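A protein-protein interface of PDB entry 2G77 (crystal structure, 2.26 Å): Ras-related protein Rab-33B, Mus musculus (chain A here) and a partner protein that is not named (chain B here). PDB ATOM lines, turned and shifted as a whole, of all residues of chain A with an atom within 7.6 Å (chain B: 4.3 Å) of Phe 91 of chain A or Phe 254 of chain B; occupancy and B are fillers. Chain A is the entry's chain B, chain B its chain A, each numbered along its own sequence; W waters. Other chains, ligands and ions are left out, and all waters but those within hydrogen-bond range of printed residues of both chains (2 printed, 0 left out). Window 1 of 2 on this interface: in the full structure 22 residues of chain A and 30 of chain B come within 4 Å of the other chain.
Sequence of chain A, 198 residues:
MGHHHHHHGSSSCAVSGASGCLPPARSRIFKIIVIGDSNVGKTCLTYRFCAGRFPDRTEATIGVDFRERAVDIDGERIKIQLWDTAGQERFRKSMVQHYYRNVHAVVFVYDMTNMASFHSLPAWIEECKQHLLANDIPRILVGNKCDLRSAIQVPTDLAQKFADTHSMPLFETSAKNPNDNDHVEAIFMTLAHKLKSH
Arg 255 of chain B touches Ile 62 of chain A. CG2 of Ile 62 of chain A touches ND2 of Asn 258 of chain B, at 3.6 Å. Phe 254 of chain B touches Gly 63 of chain A. Phe 254 of chain B touches Phe 91 of chain A. Ser 94 of chain A touches Gln 217 of chain B (OG to OE1, 3.7 Å). Phe 254 of chain B touches Tyr 99 of chain A (CB to OH, 3.9 Å).
The backbone carbonyl oxygen of Ile 250 of chain B sits at hydrogen-bond distance from the side-chain hydroxyl of Tyr 99 of chain A. The guanidinium group (NH2) of Arg 255 of chain B lies within salt-bridge range of the side-chain carboxylate (OD1) of Asp 65 of chain A (3.3 Å).
NE2 of Gln 217 of chain B lies within hydrogen-bond range of OD1 of Asn 258 of chain B (3.0 Å). N of Ala 86 of chain A sits at hydrogen-bond distance from O of Gly 63 of chain A. N of Asp 84 of chain A sits at hydrogen-bond distance from O of Asp 65 of chain A (2.9 Å). O of Ser 94 of chain A lies within hydrogen-bond range of NE2 of Gln 97 of chain A, at 3.4 Å.
Water W2 lies within hydrogen-bond range of OH of Tyr 99 of chain A (2.4 Å), N of Val 64 of chain A (3.1 Å) and O of Ile 250 of chain B (3.3 Å). Water W1 lies within hydrogen-bond range of the side-chain carboxylate of Asp 65 of chain A (2.8 Å), the backbone NH of Ile 62 of chain A (3.1 Å) and the guanidinium group of Arg 255 of chain B (3.5 Å).
Phe 91 of chain A touches just one residue of chain B: Phe 254. Of chain A, only Gly 63, Phe 91 and Tyr 99 come within 4 Å of Phe 254 of chain B. No residue of chain A comes within 4 Å of Ala 253 of chain B. Of the printed residues of chain A, Asn 258 of chain B touches Ile 62 (3.6 Å). Of the printed residues of chain B, Gly 63 of chain A touches Phe 254. Printed residues of chain B within 4 Å of Ile 62 of chain A: Arg 255 and Asn 258. The nearest residue of chain B that does not touch Phe 91 of chain A is Gln 217 of chain B (4.2 Å). The nearest printed residue of chain B that does not touch Asp 65 of chain A is Phe 252 of chain B (8.5 Å).
Of the 22 printed residues of chain A, 6 touch a printed residue of chain B. Of the 11 printed residues of chain B, 5 touch a printed residue of chain A. Hydrophobic or aromatic side chains of chain B within 4 Å of the printed part of chain A: Ile 250 and Phe 254. Along chain B the printed residues that touch a printed residue of chain A span positions 217 to 258. Among the printed residues, 8 pairs touch across the chains. Among the printed residues, Asp or Glu carboxylates within 4 Å of a Lys or Arg side-chain nitrogen of the other chain: Asp 65 of chain A with Arg 255 of chain B (3.3 Å).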
ATOM      1  N   THR A  61       1.341 -16.615 -26.876  1.00  0.00           N
ATOM      2  CA  THR A  61       1.857 -16.170 -25.570  1.00  0.00           C
ATOM      3  C   THR A  61       3.067 -17.017 -25.190  1.00  0.00           C
ATOM      4  O   THR A  61       3.043 -18.258 -25.354  1.00  0.00           O
ATOM      5  CB  THR A  61       0.755 -16.297 -24.447  1.00  0.00           C
ATOM      6  OG1 THR A  61      -0.440 -15.590 -24.880  1.00  0.00           O
ATOM      7  CG2 THR A  61       1.253 -15.847 -23.050  1.00  0.00           C
ATOM      8  N   ILE A  62       4.109 -16.342 -24.667  1.00  0.00           N
ATOM      9  CA  ILE A  62       5.367 -16.979 -24.315  1.00  0.00           C
ATOM     10  C   ILE A  62       5.566 -16.728 -22.839  1.00  0.00           C
ATOM     11  O   ILE A  62       5.627 -15.585 -22.415  1.00  0.00           O
ATOM     12  CB  ILE A  62       6.581 -16.374 -25.103  1.00  0.00           C
ATOM     13  CG1 ILE A  62       6.378 -16.512 -26.645  1.00  0.00           C
ATOM     14  CG2 ILE A  62       7.923 -17.077 -24.666  1.00  0.00           C
ATOM     15  CD1 ILE A  62       6.205 -17.973 -27.178  1.00  0.00           C
ATOM     16  N   GLY A  63       5.678 -17.778 -22.049  1.00  0.00           N
ATOM     17  CA  GLY A  63       5.724 -17.569 -20.605  1.00  0.00           C
ATOM     18  C   GLY A  63       4.320 -17.252 -20.123  1.00  0.00           C
ATOM     19  O   GLY A  63       3.359 -18.005 -20.432  1.00  0.00           O
ATOM     20  N   VAL A  64       4.189 -16.210 -19.306  1.00  0.00           N
ATOM     21  CA  VAL A  64       2.925 -15.935 -18.653  1.00  0.00           C
ATOM     22  C   VAL A  64       2.690 -14.444 -18.666  1.00  0.00           C
ATOM     23  O   VAL A  64       3.417 -13.717 -18.013  1.00  0.00           O
ATOM     24  CB  VAL A  64       2.837 -16.490 -17.177  1.00  0.00           C
ATOM     25  CG1 VAL A  64       1.419 -16.235 -16.656  1.00  0.00           C
ATOM     26  CG2 VAL A  64       3.174 -18.013 -17.071  1.00  0.00           C
ATOM     27  N   ASP A  65       1.695 -13.994 -19.423  1.00  0.00           N
ATOM     28  CA  ASP A  65       1.372 -12.586 -19.554  1.00  0.00           C
ATOM     29  C   ASP A  65       0.622 -12.103 -18.329  1.00  0.00           C
ATOM     30  O   ASP A  65      -0.222 -12.822 -17.768  1.00  0.00           O
ATOM     31  CB  ASP A  65       0.513 -12.356 -20.822  1.00  0.00           C
ATOM     32  CG  ASP A  65       1.354 -12.219 -22.104  1.00  0.00           C
ATOM     33  OD1 ASP A  65       2.599 -12.442 -22.102  1.00  0.00           O
ATOM     34  OD2 ASP A  65       0.753 -11.871 -23.140  1.00  0.00           O
ATOM     35  N   ASP A  84      -2.203 -14.954 -17.689  1.00  0.00           N
ATOM     36  CA  ASP A  84      -2.561 -15.680 -18.890  1.00  0.00           C
ATOM     37  C   ASP A  84      -1.375 -16.561 -19.349  1.00  0.00           C
ATOM     38  O   ASP A  84      -0.354 -16.034 -19.816  1.00  0.00           O
ATOM     39  CB  ASP A  84      -2.994 -14.667 -19.963  1.00  0.00           C
ATOM     40  CG  ASP A  84      -3.021 -15.247 -21.287  1.00  0.00           C
ATOM     41  OD1 ASP A  84      -3.253 -16.501 -21.360  1.00  0.00           O
ATOM     42  OD2 ASP A  84      -2.790 -14.479 -22.278  1.00  0.00           O
ATOM     43  N   THR A  85      -1.494 -17.892 -19.229  1.00  0.00           N
ATOM     44  CA  THR A  85      -0.342 -18.753 -19.510  1.00  0.00           C
ATOM     45  C   THR A  85      -0.185 -19.167 -20.974  1.00  0.00           C
ATOM     46  O   THR A  85      -1.174 -19.148 -21.748  1.00  0.00           O
ATOM     47  CB  THR A  85      -0.345 -20.080 -18.696  1.00  0.00           C
ATOM     48  OG1 THR A  85      -1.495 -20.876 -19.086  1.00  0.00           O
ATOM     49  CG2 THR A  85      -0.374 -19.798 -17.196  1.00  0.00           C
ATOM     50  N   ALA A  86       1.051 -19.548 -21.336  1.00  0.00           N
ATOM     51  CA  ALA A  86       1.318 -20.292 -22.568  1.00  0.00           C
ATOM     52  C   ALA A  86       0.866 -21.725 -22.343  1.00  0.00           C
ATOM     53  O   ALA A  86       1.133 -22.305 -21.282  1.00  0.00           O
ATOM     54  CB  ALA A  86       2.810 -20.272 -22.942  1.00  0.00           C
ATOM     55  N   GLY A  87       0.235 -22.308 -23.364  1.00  0.00           N
ATOM     56  CA  GLY A  87      -0.449 -23.554 -23.203  1.00  0.00           C
ATOM     57  C   GLY A  87       0.227 -24.740 -23.828  1.00  0.00           C
ATOM     58  O   GLY A  87      -0.304 -25.827 -23.697  1.00  0.00           O
ATOM     59  N   GLN A  88       1.370 -24.565 -24.525  1.00  0.00           N
ATOM     60  CA  GLN A  88       2.053 -25.749 -25.078  1.00  0.00           C
ATOM     61  C   GLN A  88       2.586 -26.670 -23.960  1.00  0.00           C
ATOM     62  O   GLN A  88       3.071 -26.192 -22.909  1.00  0.00           O
ATOM     63  CB  GLN A  88       3.163 -25.369 -26.032  1.00  0.00           C
ATOM     64  CG  GLN A  88       3.623 -26.540 -26.901  1.00  0.00           C
ATOM     65  CD  GLN A  88       4.810 -26.177 -27.775  1.00  0.00           C
ATOM     66  OE1 GLN A  88       5.577 -25.257 -27.467  1.00  0.00           O
ATOM     67  NE2 GLN A  88       4.975 -26.905 -28.876  1.00  0.00           N
ATOM     68  N   GLU A  89       2.475 -27.981 -24.172  1.00  0.00           N
ATOM     69  CA  GLU A  89       2.984 -28.967 -23.177  1.00  0.00           C
ATOM     70  C   GLU A  89       4.404 -28.644 -22.681  1.00  0.00           C
ATOM     71  O   GLU A  89       4.672 -28.627 -21.460  1.00  0.00           O
ATOM     72  CB  GLU A  89       2.948 -30.411 -23.710  1.00  0.00           C
ATOM     73  CG  GLU A  89       3.388 -31.366 -22.587  1.00  0.00           C
ATOM     74  CD  GLU A  89       3.179 -32.855 -22.872  1.00  0.00           C
ATOM     75  OE1 GLU A  89       2.486 -33.197 -23.887  1.00  0.00           O
ATOM     76  OE2 GLU A  89       3.732 -33.687 -22.073  1.00  0.00           O
ATOM     77  N   ARG A  90       5.321 -28.374 -23.610  1.00  0.00           N
ATOM     78  CA  ARG A  90       6.685 -28.043 -23.219  1.00  0.00           C
ATOM     79  C   ARG A  90       6.795 -27.030 -22.073  1.00  0.00           C
ATOM     80  O   ARG A  90       7.615 -27.191 -21.130  1.00  0.00           O
ATOM     81  CB  ARG A  90       7.489 -27.533 -24.433  1.00  0.00           C
ATOM     82  CG  ARG A  90       8.895 -27.107 -24.062  1.00  0.00           C
ATOM     83  CD  ARG A  90       9.721 -28.327 -23.541  1.00  0.00           C
ATOM     84  NE  ARG A  90      10.250 -29.038 -24.673  1.00  0.00           N
ATOM     85  CZ  ARG A  90       9.992 -30.299 -24.971  1.00  0.00           C
ATOM     86  NH1 ARG A  90       9.246 -31.050 -24.186  1.00  0.00           N
ATOM     87  NH2 ARG A  90      10.536 -30.818 -26.056  1.00  0.00           N
ATOM     88  N   PHE A  91       6.022 -25.952 -22.173  1.00  0.00           N
ATOM     89  CA  PHE A  91       6.098 -24.912 -21.159  1.00  0.00           C
ATOM     90  C   PHE A  91       5.430 -25.406 -19.865  1.00  0.00           C
ATOM     91  O   PHE A  91       5.964 -25.195 -18.769  1.00  0.00           O
ATOM     92  CB  PHE A  91       5.488 -23.597 -21.658  1.00  0.00           C
ATOM     93  CG  PHE A  91       5.307 -22.581 -20.582  1.00  0.00           C
ATOM     94  CD1 PHE A  91       6.346 -21.714 -20.241  1.00  0.00           C
ATOM     95  CD2 PHE A  91       4.110 -22.498 -19.880  1.00  0.00           C
ATOM     96  CE1 PHE A  91       6.194 -20.777 -19.213  1.00  0.00           C
ATOM     97  CE2 PHE A  91       3.951 -21.568 -18.869  1.00  0.00           C
ATOM     98  CZ  PHE A  91       4.996 -20.709 -18.528  1.00  0.00           C
ATOM     99  N   ARG A  92       4.285 -26.081 -20.019  1.00  0.00           N
ATOM    100  CA  ARG A  92       3.514 -26.672 -18.917  1.00  0.00           C
ATOM    101  C   ARG A  92       4.410 -27.404 -17.919  1.00  0.00           C
ATOM    102  O   ARG A  92       4.447 -27.052 -16.747  1.00  0.00           O
ATOM    103  CB  ARG A  92       2.464 -27.644 -19.478  1.00  0.00           C
ATOM    104  CG  ARG A  92       1.049 -27.325 -19.068  1.00  0.00           C
ATOM    105  CD  ARG A  92       0.255 -28.572 -18.713  1.00  0.00           C
ATOM    106  NE  ARG A  92      -0.309 -29.246 -19.875  1.00  0.00           N
ATOM    107  CZ  ARG A  92      -0.416 -30.561 -19.994  1.00  0.00           C
ATOM    108  NH1 ARG A  92       0.029 -31.351 -19.020  1.00  0.00           N
ATOM    109  NH2 ARG A  92      -0.942 -31.083 -21.102  1.00  0.00           N
ATOM    110  N   LYS A  93       5.157 -28.388 -18.437  1.00  0.00           N
ATOM    111  CA  LYS A  93       6.055 -29.282 -17.682  1.00  0.00           C
ATOM    112  C   LYS A  93       7.400 -28.626 -17.361  1.00  0.00           C
ATOM    113  O   LYS A  93       8.282 -29.255 -16.738  1.00  0.00           O
ATOM    114  CB  LYS A  93       6.336 -30.563 -18.494  1.00  0.00           C
ATOM    115  CG  LYS A  93       5.166 -31.121 -19.307  1.00  0.00           C
ATOM    116  CD  LYS A  93       4.109 -31.770 -18.413  1.00  0.00           C
ATOM    117  CE  LYS A  93       4.236 -33.274 -18.461  1.00  0.00           C
ATOM    118  NZ  LYS A  93       3.950 -33.748 -19.848  1.00  0.00           N
ATOM    119  N   SER A  94       7.581 -27.394 -17.833  1.00  0.00           N
ATOM    120  CA  SER A  94       8.790 -26.632 -17.573  1.00  0.00           C
ATOM    121  C   SER A  94       8.580 -25.747 -16.368  1.00  0.00           C
ATOM    122  O   SER A  94       9.280 -25.898 -15.375  1.00  0.00           O
ATOM    123  CB  SER A  94       9.228 -25.798 -18.812  1.00  0.00           C
ATOM    124  OG  SER A  94       9.894 -24.573 -18.460  1.00  0.00           O
ATOM    125  N   MET A  95       7.607 -24.834 -16.457  1.00  0.00           N
ATOM    126  CA  MET A  95       7.529 -23.712 -15.506  1.00  0.00           C
ATOM    127  C   MET A  95       6.144 -23.283 -15.019  1.00  0.00           C
ATOM    128  O   MET A  95       6.050 -22.735 -13.905  1.00  0.00           O
ATOM    129  CB  MET A  95       8.318 -22.479 -16.013  1.00  0.00           C
ATOM    130  N   VAL A  96       5.082 -23.507 -15.812  1.00  0.00           N
ATOM    131  CA  VAL A  96       3.727 -23.062 -15.389  1.00  0.00           C
ATOM    132  C   VAL A  96       3.524 -23.372 -13.895  1.00  0.00           C
ATOM    133  O   VAL A  96       2.950 -22.558 -13.167  1.00  0.00           O
ATOM    134  CB  VAL A  96       2.538 -23.601 -16.263  1.00  0.00           C
ATOM    135  CG1 VAL A  96       2.258 -25.081 -16.002  1.00  0.00           C
ATOM    136  CG2 VAL A  96       1.291 -22.809 -15.971  1.00  0.00           C
ATOM    137  N   GLN A  97       4.041 -24.541 -13.478  1.00  0.00           N
ATOM    138  CA  GLN A  97       4.121 -25.017 -12.082  1.00  0.00           C
ATOM    139  C   GLN A  97       4.534 -23.983 -11.016  1.00  0.00           C
ATOM    140  O   GLN A  97       3.920 -23.924  -9.948  1.00  0.00           O
ATOM    141  CB  GLN A  97       5.070 -26.215 -12.007  1.00  0.00           C
ATOM    142  CG  GLN A  97       6.429 -25.986 -12.677  1.00  0.00           C
ATOM    143  CD  GLN A  97       7.549 -26.665 -11.920  1.00  0.00           C
ATOM    144  OE1 GLN A  97       7.781 -26.384 -10.735  1.00  0.00           O
ATOM    145  NE2 GLN A  97       8.247 -27.573 -12.592  1.00  0.00           N
ATOM    146  N   TYR A  99       4.348 -20.734 -11.417  1.00  0.00           N
ATOM    147  CA  TYR A  99       3.452 -19.580 -11.430  1.00  0.00           C
ATOM    148  C   TYR A  99       2.158 -19.961 -10.686  1.00  0.00           C
ATOM    149  O   TYR A  99       1.213 -19.172 -10.631  1.00  0.00           O
ATOM    150  CB  TYR A  99       3.138 -19.101 -12.855  1.00  0.00           C
ATOM    151  CG  TYR A  99       4.319 -18.628 -13.690  1.00  0.00           C
ATOM    152  CD1 TYR A  99       4.733 -17.275 -13.700  1.00  0.00           C
ATOM    153  CD2 TYR A  99       5.005 -19.531 -14.510  1.00  0.00           C
ATOM    154  CE1 TYR A  99       5.814 -16.852 -14.507  1.00  0.00           C
ATOM    155  CE2 TYR A  99       6.090 -19.118 -15.318  1.00  0.00           C
ATOM    156  CZ  TYR A  99       6.487 -17.788 -15.320  1.00  0.00           C
ATOM    157  OH  TYR A  99       7.558 -17.452 -16.149  1.00  0.00           O
ATOM    158  N   TRP A 124      -4.582 -30.914 -17.012  1.00  0.00           N
ATOM    159  CA  TRP A 124      -4.436 -29.577 -16.411  1.00  0.00           C
ATOM    160  C   TRP A 124      -4.848 -29.596 -14.959  1.00  0.00           C
ATOM    161  O   TRP A 124      -4.214 -28.952 -14.116  1.00  0.00           O
ATOM    162  CB  TRP A 124      -5.239 -28.491 -17.145  1.00  0.00           C
ATOM    163  CG  TRP A 124      -4.651 -28.116 -18.498  1.00  0.00           C
ATOM    164  CD1 TRP A 124      -5.066 -28.532 -19.703  1.00  0.00           C
ATOM    165  CD2 TRP A 124      -3.518 -27.288 -18.727  1.00  0.00           C
ATOM    166  NE1 TRP A 124      -4.289 -27.991 -20.710  1.00  0.00           N
ATOM    167  CE2 TRP A 124      -3.334 -27.204 -20.125  1.00  0.00           C
ATOM    168  CE3 TRP A 124      -2.668 -26.557 -17.886  1.00  0.00           C
ATOM    169  CZ2 TRP A 124      -2.297 -26.459 -20.708  1.00  0.00           C
ATOM    170  CZ3 TRP A 124      -1.678 -25.782 -18.451  1.00  0.00           C
ATOM    171  CH2 TRP A 124      -1.493 -25.738 -19.874  1.00  0.00           C
ATOM    172  N   GLU A 127      -2.194 -31.414 -12.804  1.00  0.00           N
ATOM    173  CA  GLU A 127      -1.168 -30.404 -12.689  1.00  0.00           C
ATOM    174  C   GLU A 127      -1.452 -29.351 -11.619  1.00  0.00           C
ATOM    175  O   GLU A 127      -0.555 -28.978 -10.882  1.00  0.00           O
ATOM    176  CB  GLU A 127      -0.984 -29.744 -14.051  1.00  0.00           C
ATOM    177  CG  GLU A 127       0.246 -28.890 -14.184  1.00  0.00           C
ATOM    178  CD  GLU A 127       1.085 -29.315 -15.356  1.00  0.00           C
ATOM    179  OE1 GLU A 127       0.566 -30.071 -16.227  1.00  0.00           O
ATOM    180  OE2 GLU A 127       2.274 -28.909 -15.394  1.00  0.00           O
ATOM    181  N   GLN B 217      13.237 -27.117 -20.442  1.00  0.00           N
ATOM    182  CA  GLN B 217      13.939 -25.858 -20.864  1.00  0.00           C
ATOM    183  C   GLN B 217      15.051 -25.398 -19.892  1.00  0.00           C
ATOM    184  O   GLN B 217      15.088 -24.223 -19.501  1.00  0.00           O
ATOM    185  CB  GLN B 217      12.899 -24.751 -21.100  1.00  0.00           C
ATOM    186  CG  GLN B 217      11.965 -25.133 -22.295  1.00  0.00           C
ATOM    187  CD  GLN B 217      11.073 -24.005 -22.694  1.00  0.00           C
ATOM    188  OE1 GLN B 217      10.015 -23.791 -22.099  1.00  0.00           O
ATOM    189  NE2 GLN B 217      11.492 -23.263 -23.681  1.00  0.00           N
ATOM    190  N   ILE B 220      16.939 -22.099 -20.562  1.00  0.00           N
ATOM    191  CA  ILE B 220      16.313 -20.858 -20.164  1.00  0.00           C
ATOM    192  C   ILE B 220      16.410 -20.635 -18.668  1.00  0.00           C
ATOM    193  O   ILE B 220      16.724 -19.502 -18.227  1.00  0.00           O
ATOM    194  CB  ILE B 220      14.896 -20.817 -20.620  1.00  0.00           C
ATOM    195  CG1 ILE B 220      14.911 -20.751 -22.171  1.00  0.00           C
ATOM    196  CG2 ILE B 220      14.176 -19.630 -19.923  1.00  0.00           C
ATOM    197  CD1 ILE B 220      13.618 -20.505 -22.695  1.00  0.00           C
ATOM    198  N   VAL B 224      18.079 -17.393 -16.831  1.00  0.00           N
ATOM    199  CA  VAL B 224      17.391 -16.517 -15.917  1.00  0.00           C
ATOM    200  C   VAL B 224      18.144 -16.460 -14.555  1.00  0.00           C
ATOM    201  O   VAL B 224      18.278 -15.380 -13.970  1.00  0.00           O
ATOM    202  CB  VAL B 224      15.918 -16.951 -15.702  1.00  0.00           C
ATOM    203  CG1 VAL B 224      15.273 -16.077 -14.652  1.00  0.00           C
ATOM    204  CG2 VAL B 224      15.079 -16.877 -17.051  1.00  0.00           C
ATOM    205  N   ILE B 250      11.901 -14.631 -13.312  1.00  0.00           N
ATOM    206  CA  ILE B 250      11.218 -15.530 -14.201  1.00  0.00           C
ATOM    207  C   ILE B 250       9.879 -14.915 -14.684  1.00  0.00           C
ATOM    208  O   ILE B 250       9.399 -15.294 -15.707  1.00  0.00           O
ATOM    209  CB  ILE B 250      11.018 -16.927 -13.512  1.00  0.00           C
ATOM    210  CG1 ILE B 250      10.728 -18.077 -14.512  1.00  0.00           C
ATOM    211  CG2 ILE B 250       9.981 -16.855 -12.471  1.00  0.00           C
ATOM    212  CD1 ILE B 250      11.949 -18.643 -15.137  1.00  0.00           C
ATOM    213  N   PHE B 252       9.371 -12.099 -16.077  1.00  0.00           N
ATOM    214  CA  PHE B 252       9.492 -11.275 -17.266  1.00  0.00           C
ATOM    215  C   PHE B 252      10.656 -11.767 -18.104  1.00  0.00           C
ATOM    216  O   PHE B 252      10.685 -11.514 -19.286  1.00  0.00           O
ATOM    217  CB  PHE B 252       9.654  -9.770 -16.885  1.00  0.00           C
ATOM    218  CG  PHE B 252      10.882  -9.509 -16.050  1.00  0.00           C
ATOM    219  CD1 PHE B 252      12.100  -9.318 -16.651  1.00  0.00           C
ATOM    220  CD2 PHE B 252      10.808  -9.494 -14.636  1.00  0.00           C
ATOM    221  CE1 PHE B 252      13.286  -9.137 -15.870  1.00  0.00           C
ATOM    222  CE2 PHE B 252      11.966  -9.289 -13.839  1.00  0.00           C
ATOM    223  CZ  PHE B 252      13.194  -9.106 -14.455  1.00  0.00           C
ATOM    224  N   ALA B 253      11.630 -12.454 -17.500  1.00  0.00           N
ATOM    225  CA  ALA B 253      12.838 -12.821 -18.230  1.00  0.00           C
ATOM    226  C   ALA B 253      12.783 -14.175 -18.952  1.00  0.00           C
ATOM    227  O   ALA B 253      13.659 -14.490 -19.740  1.00  0.00           O
ATOM    228  CB  ALA B 253      14.087 -12.745 -17.310  1.00  0.00           C
ATOM    229  N   PHE B 254      11.755 -14.976 -18.678  1.00  0.00           N
ATOM    230  CA  PHE B 254      11.582 -16.222 -19.378  1.00  0.00           C
ATOM    231  C   PHE B 254      11.353 -15.880 -20.875  1.00  0.00           C
ATOM    232  O   PHE B 254      12.047 -16.486 -21.708  1.00  0.00           O
ATOM    233  CB  PHE B 254      10.404 -17.090 -18.825  1.00  0.00           C
ATOM    234  CG  PHE B 254      10.206 -18.393 -19.615  1.00  0.00           C
ATOM    235  CD1 PHE B 254      10.737 -19.582 -19.176  1.00  0.00           C
ATOM    236  CD2 PHE B 254       9.506 -18.398 -20.841  1.00  0.00           C
ATOM    237  CE1 PHE B 254      10.591 -20.766 -19.940  1.00  0.00           C
ATOM    238  CE2 PHE B 254       9.344 -19.550 -21.569  1.00  0.00           C
ATOM    239  CZ  PHE B 254       9.914 -20.721 -21.146  1.00  0.00           C
ATOM    240  N   ARG B 255      10.444 -14.976 -21.207  1.00  0.00           N
ATOM    241  CA  ARG B 255      10.204 -14.586 -22.610  1.00  0.00           C
ATOM    242  C   ARG B 255      11.497 -13.985 -23.206  1.00  0.00           C
ATOM    243  O   ARG B 255      11.801 -14.190 -24.365  1.00  0.00           O
ATOM    244  CB  ARG B 255       9.020 -13.617 -22.654  1.00  0.00           C
ATOM    245  CG  ARG B 255       8.298 -13.305 -23.997  1.00  0.00           C
ATOM    246  CD  ARG B 255       8.120 -11.815 -24.060  1.00  0.00           C
ATOM    247  NE  ARG B 255       6.779 -11.486 -23.714  1.00  0.00           N
ATOM    248  CZ  ARG B 255       6.252 -10.322 -23.391  1.00  0.00           C
ATOM    249  NH1 ARG B 255       6.905  -9.171 -23.370  1.00  0.00           N
ATOM    250  NH2 ARG B 255       4.957 -10.351 -23.134  1.00  0.00           N
ATOM    251  N   TRP B 256      12.306 -13.301 -22.371  1.00  0.00           N
ATOM    252  CA  TRP B 256      13.551 -12.615 -22.848  1.00  0.00           C
ATOM    253  C   TRP B 256      14.501 -13.648 -23.358  1.00  0.00           C
ATOM    254  O   TRP B 256      15.149 -13.468 -24.401  1.00  0.00           O
ATOM    255  CB  TRP B 256      14.256 -11.818 -21.737  1.00  0.00           C
ATOM    256  CG  TRP B 256      13.537 -10.542 -21.354  1.00  0.00           C
ATOM    257  CD1 TRP B 256      12.297 -10.161 -21.734  1.00  0.00           C
ATOM    258  CD2 TRP B 256      14.012  -9.531 -20.463  1.00  0.00           C
ATOM    259  NE1 TRP B 256      11.983  -8.945 -21.183  1.00  0.00           N
ATOM    260  CE2 TRP B 256      13.035  -8.537 -20.405  1.00  0.00           C
ATOM    261  CE3 TRP B 256      15.219  -9.338 -19.771  1.00  0.00           C
ATOM    262  CZ2 TRP B 256      13.187  -7.369 -19.629  1.00  0.00           C
ATOM    263  CZ3 TRP B 256      15.373  -8.182 -19.000  1.00  0.00           C
ATOM    264  CH2 TRP B 256      14.373  -7.202 -18.958  1.00  0.00           C
ATOM    265  N   MET B 257      14.582 -14.764 -22.671  1.00  0.00           N
ATOM    266  CA  MET B 257      15.484 -15.852 -23.150  1.00  0.00           C
ATOM    267  C   MET B 257      14.875 -16.676 -24.257  1.00  0.00           C
ATOM    268  O   MET B 257      15.556 -17.027 -25.172  1.00  0.00           O
ATOM    269  CB  MET B 257      15.870 -16.776 -21.990  1.00  0.00           C
ATOM    270  CG  MET B 257      16.391 -16.017 -20.728  1.00  0.00           C
ATOM    271  SD  MET B 257      17.805 -14.927 -21.200  1.00  0.00           S
ATOM    272  CE  MET B 257      17.892 -13.939 -19.661  1.00  0.00           C
ATOM    273  N   ASN B 258      13.588 -17.012 -24.145  1.00  0.00           N
ATOM    274  CA  ASN B 258      12.972 -17.960 -25.080  1.00  0.00           C
ATOM    275  C   ASN B 258      12.937 -17.345 -26.501  1.00  0.00           C
ATOM    276  O   ASN B 258      13.142 -18.050 -27.480  1.00  0.00           O
ATOM    277  CB  ASN B 258      11.576 -18.305 -24.581  1.00  0.00           C
ATOM    278  CG  ASN B 258      10.928 -19.420 -25.348  1.00  0.00           C
ATOM    279  OD1 ASN B 258      11.016 -20.534 -24.915  1.00  0.00           O
ATOM    280  ND2 ASN B 258      10.243 -19.129 -26.484  1.00  0.00           N
HETATM  281  O   HOH W   1       3.612 -13.241 -24.550  1.00  0.00           O
HETATM  282  O   HOH W   2       6.927 -15.779 -17.823  1.00  0.00           O
